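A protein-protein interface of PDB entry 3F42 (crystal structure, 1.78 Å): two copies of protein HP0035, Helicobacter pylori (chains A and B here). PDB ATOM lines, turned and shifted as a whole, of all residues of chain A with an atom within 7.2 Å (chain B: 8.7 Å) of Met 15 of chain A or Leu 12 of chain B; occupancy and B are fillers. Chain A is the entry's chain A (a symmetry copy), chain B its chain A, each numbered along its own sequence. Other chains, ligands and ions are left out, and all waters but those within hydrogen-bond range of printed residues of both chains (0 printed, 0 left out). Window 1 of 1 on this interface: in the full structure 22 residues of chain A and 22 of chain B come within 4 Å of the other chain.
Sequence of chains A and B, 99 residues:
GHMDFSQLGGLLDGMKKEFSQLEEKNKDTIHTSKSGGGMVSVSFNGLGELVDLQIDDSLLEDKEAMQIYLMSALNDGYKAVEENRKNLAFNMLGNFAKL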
ATOM      1  N   LEU A   8     -31.993 -11.717  20.601  1.00  0.00           N
ATOM      2  CA  LEU A   8     -31.720 -12.091  19.216  1.00  0.00           C
ATOM      3  C   LEU A   8     -30.227 -12.253  18.971  1.00  0.00           C
ATOM      4  O   LEU A   8     -29.811 -13.198  18.294  1.00  0.00           O
ATOM      5  CB  LEU A   8     -32.311 -11.066  18.235  1.00  0.00           C
ATOM      6  CG  LEU A   8     -31.983 -11.196  16.735  1.00  0.00           C
ATOM      7  CD1 LEU A   8     -32.420 -12.584  16.221  1.00  0.00           C
ATOM      8  CD2 LEU A   8     -32.669 -10.058  15.907  1.00  0.00           C
ATOM      9  N   GLY A   9     -29.424 -11.345  19.519  1.00  0.00           N
ATOM     10  CA  GLY A   9     -27.969 -11.426  19.342  1.00  0.00           C
ATOM     11  C   GLY A   9     -27.416 -12.687  19.995  1.00  0.00           C
ATOM     12  O   GLY A   9     -26.523 -13.345  19.433  1.00  0.00           O
ATOM     13  N   GLY A  10     -27.955 -13.031  21.158  1.00  0.00           N
ATOM     14  CA  GLY A  10     -27.578 -14.259  21.881  1.00  0.00           C
ATOM     15  C   GLY A  10     -27.942 -15.515  21.075  1.00  0.00           C
ATOM     16  O   GLY A  10     -27.141 -16.475  20.973  1.00  0.00           O
ATOM     17  N   LEU A  11     -29.149 -15.518  20.511  1.00  0.00           N
ATOM     18  CA  LEU A  11     -29.560 -16.616  19.620  1.00  0.00           C
ATOM     19  C   LEU A  11     -28.657 -16.747  18.401  1.00  0.00           C
ATOM     20  O   LEU A  11     -28.235 -17.870  18.046  1.00  0.00           O
ATOM     21  CB  LEU A  11     -31.001 -16.412  19.167  1.00  0.00           C
ATOM     22  CG  LEU A  11     -31.647 -17.722  18.752  1.00  0.00           C
ATOM     23  CD1 LEU A  11     -32.216 -18.373  20.047  1.00  0.00           C
ATOM     24  CD2 LEU A  11     -32.722 -17.408  17.718  1.00  0.00           C
ATOM     25  N   LEU A  12     -28.353 -15.623  17.748  1.00  0.00           N
ATOM     26  CA  LEU A  12     -27.485 -15.639  16.566  1.00  0.00           C
ATOM     27  C   LEU A  12     -26.107 -16.189  16.940  1.00  0.00           C
ATOM     28  O   LEU A  12     -25.536 -17.023  16.204  1.00  0.00           O
ATOM     29  CB  LEU A  12     -27.336 -14.253  15.947  1.00  0.00           C
ATOM     30  CG  LEU A  12     -28.550 -13.688  15.202  1.00  0.00           C
ATOM     31  CD1 LEU A  12     -28.274 -12.250  14.666  1.00  0.00           C
ATOM     32  CD2 LEU A  12     -29.002 -14.576  14.042  1.00  0.00           C
ATOM     33  N   ASP A  13     -25.585 -15.754  18.087  1.00  0.00           N
ATOM     34  CA  ASP A  13     -24.255 -16.243  18.530  1.00  0.00           C
ATOM     35  C   ASP A  13     -24.265 -17.746  18.806  1.00  0.00           C
ATOM     36  O   ASP A  13     -23.327 -18.457  18.398  1.00  0.00           O
ATOM     37  CB  ASP A  13     -23.724 -15.483  19.738  1.00  0.00           C
ATOM     38  CG  ASP A  13     -23.290 -14.091  19.406  1.00  0.00           C
ATOM     39  OD1 ASP A  13     -23.037 -13.792  18.219  1.00  0.00           O
ATOM     40  OD2 ASP A  13     -23.176 -13.275  20.339  1.00  0.00           O
ATOM     41  N   GLY A  14     -25.321 -18.222  19.462  1.00  0.00           N
ATOM     42  CA  GLY A  14     -25.512 -19.643  19.773  1.00  0.00           C
ATOM     43  C   GLY A  14     -25.652 -20.472  18.496  1.00  0.00           C
ATOM     44  O   GLY A  14     -25.062 -21.569  18.365  1.00  0.00           O
ATOM     45  N   MET A  15     -26.435 -19.955  17.553  1.00  0.00           N
ATOM     46  CA  MET A  15     -26.610 -20.644  16.269  1.00  0.00           C
ATOM     47  C   MET A  15     -25.300 -20.722  15.492  1.00  0.00           C
ATOM     48  O   MET A  15     -24.997 -21.773  14.900  1.00  0.00           O
ATOM     49  CB  MET A  15     -27.709 -19.989  15.458  1.00  0.00           C
ATOM     50  CG  MET A  15     -29.034 -20.359  16.003  1.00  0.00           C
ATOM     51  SD  MET A  15     -30.356 -19.413  14.970  1.00  0.00           S
ATOM     52  CE  MET A  15     -30.452 -20.595  13.507  1.00  0.00           C
ATOM     53  N   LYS A  16     -24.492 -19.653  15.543  1.00  0.00           N
ATOM     54  CA  LYS A  16     -23.209 -19.648  14.834  1.00  0.00           C
ATOM     55  C   LYS A  16     -22.238 -20.618  15.502  1.00  0.00           C
ATOM     56  O   LYS A  16     -21.450 -21.259  14.822  1.00  0.00           O
ATOM     57  CB  LYS A  16     -22.624 -18.234  14.736  1.00  0.00           C
ATOM     58  CG  LYS A  16     -21.272 -18.172  13.968  1.00  0.00           C
ATOM     59  CD  LYS A  16     -20.483 -16.896  14.297  1.00  0.00           C
ATOM     60  CE  LYS A  16     -19.024 -17.031  13.819  1.00  0.00           C
ATOM     61  NZ  LYS A  16     -18.216 -15.814  14.130  1.00  0.00           N
ATOM     62  N   LYS A  17     -22.320 -20.744  16.822  1.00  0.00           N
ATOM     63  CA  LYS A  17     -21.482 -21.713  17.524  1.00  0.00           C
ATOM     64  C   LYS A  17     -21.835 -23.153  17.111  1.00  0.00           C
ATOM     65  O   LYS A  17     -20.938 -23.954  16.759  1.00  0.00           O
ATOM     66  CB  LYS A  17     -21.599 -21.533  19.041  1.00  0.00           C
ATOM     67  CG  LYS A  17     -20.856 -22.619  19.828  1.00  0.00           C
ATOM     68  CD  LYS A  17     -20.811 -22.245  21.310  1.00  0.00           C
ATOM     69  CE  LYS A  17     -19.922 -23.169  22.126  1.00  0.00           C
ATOM     70  NZ  LYS A  17     -20.484 -24.543  22.209  1.00  0.00           N
ATOM     71  N   GLU A  18     -23.132 -23.466  17.133  1.00  0.00           N
ATOM     72  CA  GLU A  18     -23.644 -24.767  16.711  1.00  0.00           C
ATOM     73  C   GLU A  18     -23.259 -25.035  15.255  1.00  0.00           C
ATOM     74  O   GLU A  18     -22.826 -26.170  14.909  1.00  0.00           O
ATOM     75  CB  GLU A  18     -25.170 -24.803  16.819  1.00  0.00           C
ATOM     76  CG  GLU A  18     -25.721 -26.224  16.711  1.00  0.00           C
ATOM     77  CD  GLU A  18     -27.243 -26.293  16.622  1.00  0.00           C
ATOM     78  OE1 GLU A  18     -27.950 -25.267  16.792  1.00  0.00           O
ATOM     79  OE2 GLU A  18     -27.739 -27.406  16.350  1.00  0.00           O
ATOM     80  N   PHE A  19     -23.440 -24.033  14.401  1.00  0.00           N
ATOM     81  CA  PHE A  19     -23.132 -24.186  12.987  1.00  0.00           C
ATOM     82  C   PHE A  19     -21.646 -24.597  12.812  1.00  0.00           C
ATOM     83  O   PHE A  19     -21.321 -25.524  12.040  1.00  0.00           O
ATOM     84  CB  PHE A  19     -23.423 -22.884  12.233  1.00  0.00           C
ATOM     85  CG  PHE A  19     -23.263 -22.999  10.763  1.00  0.00           C
ATOM     86  CD1 PHE A  19     -24.351 -23.332   9.968  1.00  0.00           C
ATOM     87  CD2 PHE A  19     -22.017 -22.866  10.169  1.00  0.00           C
ATOM     88  CE1 PHE A  19     -24.214 -23.483   8.600  1.00  0.00           C
ATOM     89  CE2 PHE A  19     -21.855 -23.031   8.785  1.00  0.00           C
ATOM     90  CZ  PHE A  19     -22.942 -23.341   7.994  1.00  0.00           C
ATOM     91  N   SER A  20     -20.743 -23.889  13.479  1.00  0.00           N
ATOM     92  CA  SER A  20     -19.309 -24.214  13.382  1.00  0.00           C
ATOM     93  C   SER A  20     -18.958 -25.585  13.903  1.00  0.00           C
ATOM     94  O   SER A  20     -18.096 -26.284  13.340  1.00  0.00           O
ATOM     95  CB  SER A  20     -18.476 -23.153  14.114  1.00  0.00           C
ATOM     96  OG  SER A  20     -18.707 -21.933  13.433  1.00  0.00           O
ATOM     97  N   GLN A  21     -19.615 -25.988  14.973  1.00  0.00           N
ATOM     98  CA  GLN A  21     -19.410 -27.326  15.526  1.00  0.00           C
ATOM     99  C   GLN A  21     -19.848 -28.423  14.557  1.00  0.00           C
ATOM    100  O   GLN A  21     -19.138 -29.444  14.375  1.00  0.00           O
ATOM    101  CB  GLN A  21     -20.149 -27.458  16.845  1.00  0.00           C
ATOM    102  CG  GLN A  21     -19.462 -26.659  17.948  1.00  0.00           C
ATOM    103  CD  GLN A  21     -19.989 -26.989  19.317  1.00  0.00           C
ATOM    104  OE1 GLN A  21     -21.194 -27.044  19.535  1.00  0.00           O
ATOM    105  NE2 GLN A  21     -19.081 -27.201  20.259  1.00  0.00           N
ATOM    106  N   LEU A  22     -20.993 -28.204  13.927  1.00  0.00           N
ATOM    107  CA  LEU A  22     -21.475 -29.100  12.894  1.00  0.00           C
ATOM    108  C   LEU A  22     -20.597 -29.143  11.667  1.00  0.00           C
ATOM    109  O   LEU A  22     -20.417 -30.235  11.090  1.00  0.00           O
ATOM    110  CB  LEU A  22     -22.922 -28.800  12.505  1.00  0.00           C
ATOM    111  CG  LEU A  22     -23.963 -29.092  13.598  1.00  0.00           C
ATOM    112  CD1 LEU A  22     -25.311 -28.519  13.169  1.00  0.00           C
ATOM    113  CD2 LEU A  22     -24.077 -30.588  13.873  1.00  0.00           C
ATOM    114  N   MET A  92     -31.127 -28.592  12.105  1.00  0.00           N
ATOM    115  CA  MET A  92     -30.514 -27.698  13.071  1.00  0.00           C
ATOM    116  C   MET A  92     -31.557 -26.676  13.557  1.00  0.00           C
ATOM    117  O   MET A  92     -31.724 -26.461  14.775  1.00  0.00           O
ATOM    118  CB  MET A  92     -29.293 -26.982  12.484  1.00  0.00           C
ATOM    119  CG  MET A  92     -28.734 -26.047  13.485  1.00  0.00           C
ATOM    120  SD  MET A  92     -27.215 -25.071  12.903  1.00  0.00           S
ATOM    121  CE  MET A  92     -27.743 -23.337  13.658  1.00  0.00           C
ATOM    122  N   LEU A  93     -32.260 -26.079  12.593  1.00  0.00           N
ATOM    123  CA  LEU A  93     -33.386 -25.185  12.829  1.00  0.00           C
ATOM    124  C   LEU A  93     -34.558 -25.896  13.555  1.00  0.00           C
ATOM    125  O   LEU A  93     -35.403 -25.235  14.189  1.00  0.00           O
ATOM    126  CB  LEU A  93     -33.846 -24.562  11.494  1.00  0.00           C
ATOM    127  CG  LEU A  93     -32.783 -23.759  10.720  1.00  0.00           C
ATOM    128  CD1 LEU A  93     -33.301 -23.193   9.382  1.00  0.00           C
ATOM    129  CD2 LEU A  93     -32.245 -22.636  11.581  1.00  0.00           C
ATOM    130  N   MET B   3     -33.270 -24.720   1.311  1.00  0.00           N
ATOM    131  CA  MET B   3     -32.099 -24.099   1.930  1.00  0.00           C
ATOM    132  C   MET B   3     -31.104 -25.168   2.322  1.00  0.00           C
ATOM    133  O   MET B   3     -31.497 -26.181   2.896  1.00  0.00           O
ATOM    134  CB  MET B   3     -32.503 -23.323   3.164  1.00  0.00           C
ATOM    135  CG  MET B   3     -31.428 -22.344   3.561  1.00  0.00           C
ATOM    136  SD  MET B   3     -31.659 -21.555   5.317  1.00  0.00           S
ATOM    137  CE  MET B   3     -32.562 -23.044   6.185  1.00  0.00           C
ATOM    138  N   PHE B   5     -27.047 -26.156   4.049  1.00  0.00           N
ATOM    139  CA  PHE B   5     -26.304 -25.725   5.258  1.00  0.00           C
ATOM    140  C   PHE B   5     -25.431 -24.538   4.891  1.00  0.00           C
ATOM    141  O   PHE B   5     -25.266 -23.615   5.683  1.00  0.00           O
ATOM    142  CB  PHE B   5     -25.450 -26.880   5.777  1.00  0.00           C
ATOM    143  CG  PHE B   5     -25.167 -26.819   7.260  1.00  0.00           C
ATOM    144  CD1 PHE B   5     -26.210 -26.711   8.191  1.00  0.00           C
ATOM    145  CD2 PHE B   5     -23.874 -26.912   7.725  1.00  0.00           C
ATOM    146  CE1 PHE B   5     -25.939 -26.668   9.552  1.00  0.00           C
ATOM    147  CE2 PHE B   5     -23.584 -26.850   9.106  1.00  0.00           C
ATOM    148  CZ  PHE B   5     -24.624 -26.737  10.021  1.00  0.00           C
ATOM    149  N   SER B   6     -24.875 -24.558   3.679  1.00  0.00           N
ATOM    150  CA  SER B   6     -24.049 -23.415   3.268  1.00  0.00           C
ATOM    151  C   SER B   6     -24.843 -22.108   3.204  1.00  0.00           C
ATOM    152  O   SER B   6     -24.376 -21.053   3.690  1.00  0.00           O
ATOM    153  CB  SER B   6     -23.362 -23.736   1.947  1.00  0.00           C
ATOM    154  OG  SER B   6     -22.395 -24.739   2.169  1.00  0.00           O
ATOM    155  N   GLN B   7     -26.071 -22.181   2.679  1.00  0.00           N
ATOM    156  CA  GLN B   7     -26.937 -21.013   2.632  1.00  0.00           C
ATOM    157  C   GLN B   7     -27.280 -20.549   4.038  1.00  0.00           C
ATOM    158  O   GLN B   7     -27.257 -19.353   4.307  1.00  0.00           O
ATOM    159  CB  GLN B   7     -28.201 -21.283   1.836  1.00  0.00           C
ATOM    160  CG  GLN B   7     -27.892 -21.520   0.383  1.00  0.00           C
ATOM    161  CD  GLN B   7     -29.046 -22.018  -0.403  1.00  0.00           C
ATOM    162  OE1 GLN B   7     -29.776 -22.908   0.032  1.00  0.00           O
ATOM    163  NE2 GLN B   7     -29.202 -21.486  -1.614  1.00  0.00           N
ATOM    164  N   LEU B   8     -27.551 -21.480   4.941  1.00  0.00           N
ATOM    165  CA  LEU B   8     -27.858 -21.114   6.320  1.00  0.00           C
ATOM    166  C   LEU B   8     -26.687 -20.399   6.976  1.00  0.00           C
ATOM    167  O   LEU B   8     -26.886 -19.409   7.687  1.00  0.00           O
ATOM    168  CB  LEU B   8     -28.260 -22.344   7.147  1.00  0.00           C
ATOM    169  CG  LEU B   8     -28.457 -22.187   8.668  1.00  0.00           C
ATOM    170  CD1 LEU B   8     -29.528 -21.112   8.949  1.00  0.00           C
ATOM    171  CD2 LEU B   8     -28.854 -23.550   9.329  1.00  0.00           C
ATOM    172  N   GLY B   9     -25.472 -20.888   6.740  1.00  0.00           N
ATOM    173  CA  GLY B   9     -24.282 -20.258   7.325  1.00  0.00           C
ATOM    174  C   GLY B   9     -24.101 -18.844   6.785  1.00  0.00           C
ATOM    175  O   GLY B   9     -23.738 -17.926   7.540  1.00  0.00           O
ATOM    176  N   GLY B  10     -24.370 -18.668   5.497  1.00  0.00           N
ATOM    177  CA  GLY B  10     -24.309 -17.349   4.841  1.00  0.00           C
ATOM    178  C   GLY B  10     -25.348 -16.385   5.431  1.00  0.00           C
ATOM    179  O   GLY B  10     -25.050 -15.197   5.702  1.00  0.00           O
ATOM    180  N   LEU B  11     -26.568 -16.885   5.621  1.00  0.00           N
ATOM    181  CA  LEU B  11     -27.612 -16.089   6.287  1.00  0.00           C
ATOM    182  C   LEU B  11     -27.227 -15.690   7.705  1.00  0.00           C
ATOM    183  O   LEU B  11     -27.397 -14.515   8.098  1.00  0.00           O
ATOM    184  CB  LEU B  11     -28.924 -16.865   6.315  1.00  0.00           C
ATOM    185  CG  LEU B  11     -30.119 -15.937   6.446  1.00  0.00           C
ATOM    186  CD1 LEU B  11     -30.495 -15.482   5.006  1.00  0.00           C
ATOM    187  CD2 LEU B  11     -31.236 -16.705   7.142  1.00  0.00           C
ATOM    188  N   LEU B  12     -26.712 -16.645   8.484  1.00  0.00           N
ATOM    189  CA  LEU B  12     -26.300 -16.363   9.863  1.00  0.00           C
ATOM    190  C   LEU B  12     -25.201 -15.300   9.872  1.00  0.00           C
ATOM    191  O   LEU B  12     -25.239 -14.355  10.690  1.00  0.00           O
ATOM    192  CB  LEU B  12     -25.810 -17.616  10.582  1.00  0.00           C
ATOM    193  CG  LEU B  12     -26.867 -18.653  10.976  1.00  0.00           C
ATOM    194  CD1 LEU B  12     -26.222 -19.900  11.654  1.00  0.00           C
ATOM    195  CD2 LEU B  12     -27.944 -18.082  11.900  1.00  0.00           C
ATOM    196  N   ASP B  13     -24.244 -15.428   8.953  1.00  0.00           N
ATOM    197  CA  ASP B  13     -23.142 -14.434   8.885  1.00  0.00           C
ATOM    198  C   ASP B  13     -23.657 -13.039   8.528  1.00  0.00           C
ATOM    199  O   ASP B  13     -23.230 -12.045   9.147  1.00  0.00           O
ATOM    200  CB  ASP B  13     -22.033 -14.853   7.930  1.00  0.00           C
ATOM    201  CG  ASP B  13     -21.208 -15.984   8.456  1.00  0.00           C
ATOM    202  OD1 ASP B  13     -21.214 -16.232   9.681  1.00  0.00           O
ATOM    203  OD2 ASP B  13     -20.521 -16.634   7.647  1.00  0.00           O
ATOM    204  N   GLY B  14     -24.576 -12.973   7.568  1.00  0.00           N
ATOM    205  CA  GLY B  14     -25.205 -11.723   7.130  1.00  0.00           C
ATOM    206  C   GLY B  14     -26.020 -11.092   8.259  1.00  0.00           C
ATOM    207  O   GLY B  14     -25.968  -9.861   8.490  1.00  0.00           O
ATOM    208  N   MET B  15     -26.776 -11.928   8.966  1.00  0.00           N
ATOM    209  CA  MET B  15     -27.568 -11.439  10.100  1.00  0.00           C
ATOM    210  C   MET B  15     -26.678 -10.905  11.216  1.00  0.00           C
ATOM    211  O   MET B  15     -26.993  -9.857  11.806  1.00  0.00           O
ATOM    212  CB  MET B  15     -28.510 -12.518  10.596  1.00  0.00           C
ATOM    213  CG  MET B  15     -29.655 -12.661   9.670  1.00  0.00           C
ATOM    214  SD  MET B  15     -30.742 -14.107  10.331  1.00  0.00           S
ATOM    215  CE  MET B  15     -31.709 -13.146  11.631  1.00  0.00           C
ATOM    216  N   LYS B  16     -25.540 -11.571  11.465  1.00  0.00           N
ATOM    217  CA  LYS B  16     -24.621 -11.119  12.514  1.00  0.00           C
ATOM    218  C   LYS B  16     -23.956  -9.809  12.099  1.00  0.00           C
ATOM    219  O   LYS B  16     -23.713  -8.954  12.938  1.00  0.00           O
ATOM    220  CB  LYS B  16     -23.588 -12.197  12.861  1.00  0.00           C
ATOM    221  CG  LYS B  16     -22.603 -11.773  13.990  1.00  0.00           C
ATOM    222  CD  LYS B  16     -21.322 -12.620  13.981  1.00  0.00           C
ATOM    223  CE  LYS B  16     -20.236 -11.957  14.851  1.00  0.00           C
ATOM    224  NZ  LYS B  16     -18.966 -12.743  14.860  1.00  0.00           N
ATOM    225  N   LYS B  17     -23.695  -9.645  10.806  1.00  0.00           N
ATOM    226  CA  LYS B  17     -23.136  -8.387  10.319  1.00  0.00           C
ATOM    227  C   LYS B  17     -24.125  -7.225  10.526  1.00  0.00           C
ATOM    228  O   LYS B  17     -23.754  -6.161  11.073  1.00  0.00           O
ATOM    229  CB  LYS B  17     -22.730  -8.507   8.847  1.00  0.00           C
ATOM    230  CG  LYS B  17     -22.275  -7.172   8.245  1.00  0.00           C
ATOM    231  CD  LYS B  17     -21.662  -7.410   6.865  1.00  0.00           C
ATOM    232  CE  LYS B  17     -21.007  -6.166   6.287  1.00  0.00           C
ATOM    233  NZ  LYS B  17     -22.010  -5.116   5.962  1.00  0.00           N
ATOM    234  N   GLU B  18     -25.374  -7.441  10.111  1.00  0.00           N
ATOM    235  CA  GLU B  18     -26.450  -6.469  10.288  1.00  0.00           C
ATOM    236  C   GLU B  18     -26.639  -6.161  11.774  1.00  0.00           C
ATOM    237  O   GLU B  18     -26.802  -4.970  12.162  1.00  0.00           O
ATOM    238  CB  GLU B  18     -27.768  -7.024   9.741  1.00  0.00           C
ATOM    239  CG  GLU B  18     -28.834  -5.938   9.599  1.00  0.00           C
ATOM    240  CD  GLU B  18     -30.217  -6.472   9.241  1.00  0.00           C
ATOM    241  OE1 GLU B  18     -30.387  -7.680   8.935  1.00  0.00           O
ATOM    242  OE2 GLU B  18     -31.163  -5.658   9.291  1.00  0.00           O
ATOM    243  N   PHE B  19     -26.654  -7.204  12.598  1.00  0.00           N
ATOM    244  CA  PHE B  19     -26.854  -7.028  14.029  1.00  0.00           C
ATOM    245  C   PHE B  19     -25.764  -6.083  14.601  1.00  0.00           C
ATOM    246  O   PHE B  19     -26.064  -5.150  15.376  1.00  0.00           O
ATOM    247  CB  PHE B  19     -26.820  -8.383  14.743  1.00  0.00           C
ATOM    248  CG  PHE B  19     -27.149  -8.304  16.187  1.00  0.00           C
ATOM    249  CD1 PHE B  19     -28.460  -8.468  16.612  1.00  0.00           C
ATOM    250  CD2 PHE B  19     -26.180  -7.976  17.123  1.00  0.00           C
ATOM    251  CE1 PHE B  19     -28.795  -8.358  17.949  1.00  0.00           C
ATOM    252  CE2 PHE B  19     -26.502  -7.845  18.482  1.00  0.00           C
ATOM    253  CZ  PHE B  19     -27.803  -8.030  18.905  1.00  0.00           C
ATOM    254  N   MET B  92     -35.815  -6.141  12.295  1.00  0.00           N
ATOM    255  CA  MET B  92     -34.652  -6.667  11.603  1.00  0.00           C
ATOM    256  C   MET B  92     -35.027  -7.982  10.898  1.00  0.00           C
ATOM    257  O   MET B  92     -34.736  -8.172   9.699  1.00  0.00           O
ATOM    258  CB  MET B  92     -33.476  -6.885  12.560  1.00  0.00           C
ATOM    259  CG  MET B  92     -32.333  -7.466  11.821  1.00  0.00           C
ATOM    260  SD  MET B  92     -30.793  -7.808  12.875  1.00  0.00           S
ATOM    261  CE  MET B  92     -30.362  -9.561  12.105  1.00  0.00           C
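Of the 17 printed residues of chain B, 7 touch a printed residue of chain A.
Hydrophobic or aromatic side chains of chain B that line the printed part of chain A: Met 3, Phe 5, Leu 12, Met 15 and Phe 19.
Among the printed residues, merely in contact across the chains: Phe 19 of chain A with Phe 5 of chain B (3.1 Å), Leu 93 of chain A with Met 3 of chain B (3.3 Å), Phe 19 of chain A with Gly 9 of chain B (3.4 Å), Gly 9 of chain A with Phe 19 of chain B (3.4 Å), Leu 22 of chain A with Phe 5 of chain B (3.7 Å), Leu 12 of chain A with Met 15 of chain B (3.9 Å), Met 15 of chain A with Leu 12 of chain B (3.9 Å) and Met 92 of chain A with Phe 5 of chain B (3.9 Å).
NZ of Lys 16 of chain B lies close to NZ of Lys 16 of chain A (3.2 Å).
Gly 9 of chain A touches Phe 19 of chain B, and with the chains exchanged Phe 19 of chain A touches Gly 9 of chain B.
Leu 12 of chain A touches Met 15 of chain B, and with the chains exchanged Met 15 of chain A touches Leu 12 of chain B.
Lys 16 of chain A touches its own counterpart, Lys 16 of chain B.
13 positions are printed for both chains.
Of the 9 pairs that touch across the chains among the printed residues, 5 have their exchanged pair printed and touching as well.
Of the printed residues of chain B, Met 15 of chain A touches Leu 12.
Of chain A, only Met 15 comes within 4 Å of Leu 12 of chain B.
No residue of chain B comes within 4 Å of Gly 14 of chain A.
Of the printed residues of chain B, Leu 93 of chain A touches Met 3.
Of the printed residues of chain B, Phe 19 of chain A touches Phe 5 and Gly 9.
Printed residues of chain A within 4 Å of Gly 9 of chain B: Phe 19 (3.4 Å).
Lys 17 of chain B touches none of the printed residues of chain A.
The nearest residue of chain A that does not touch Leu 12 of chain B is Phe 19 of chain A (4.1 Å).
The backbone carbonyl oxygen of Lys 16 of chain A lies within hydrogen-bond range of the side-chain hydroxyl of Ser 20 of chain A.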
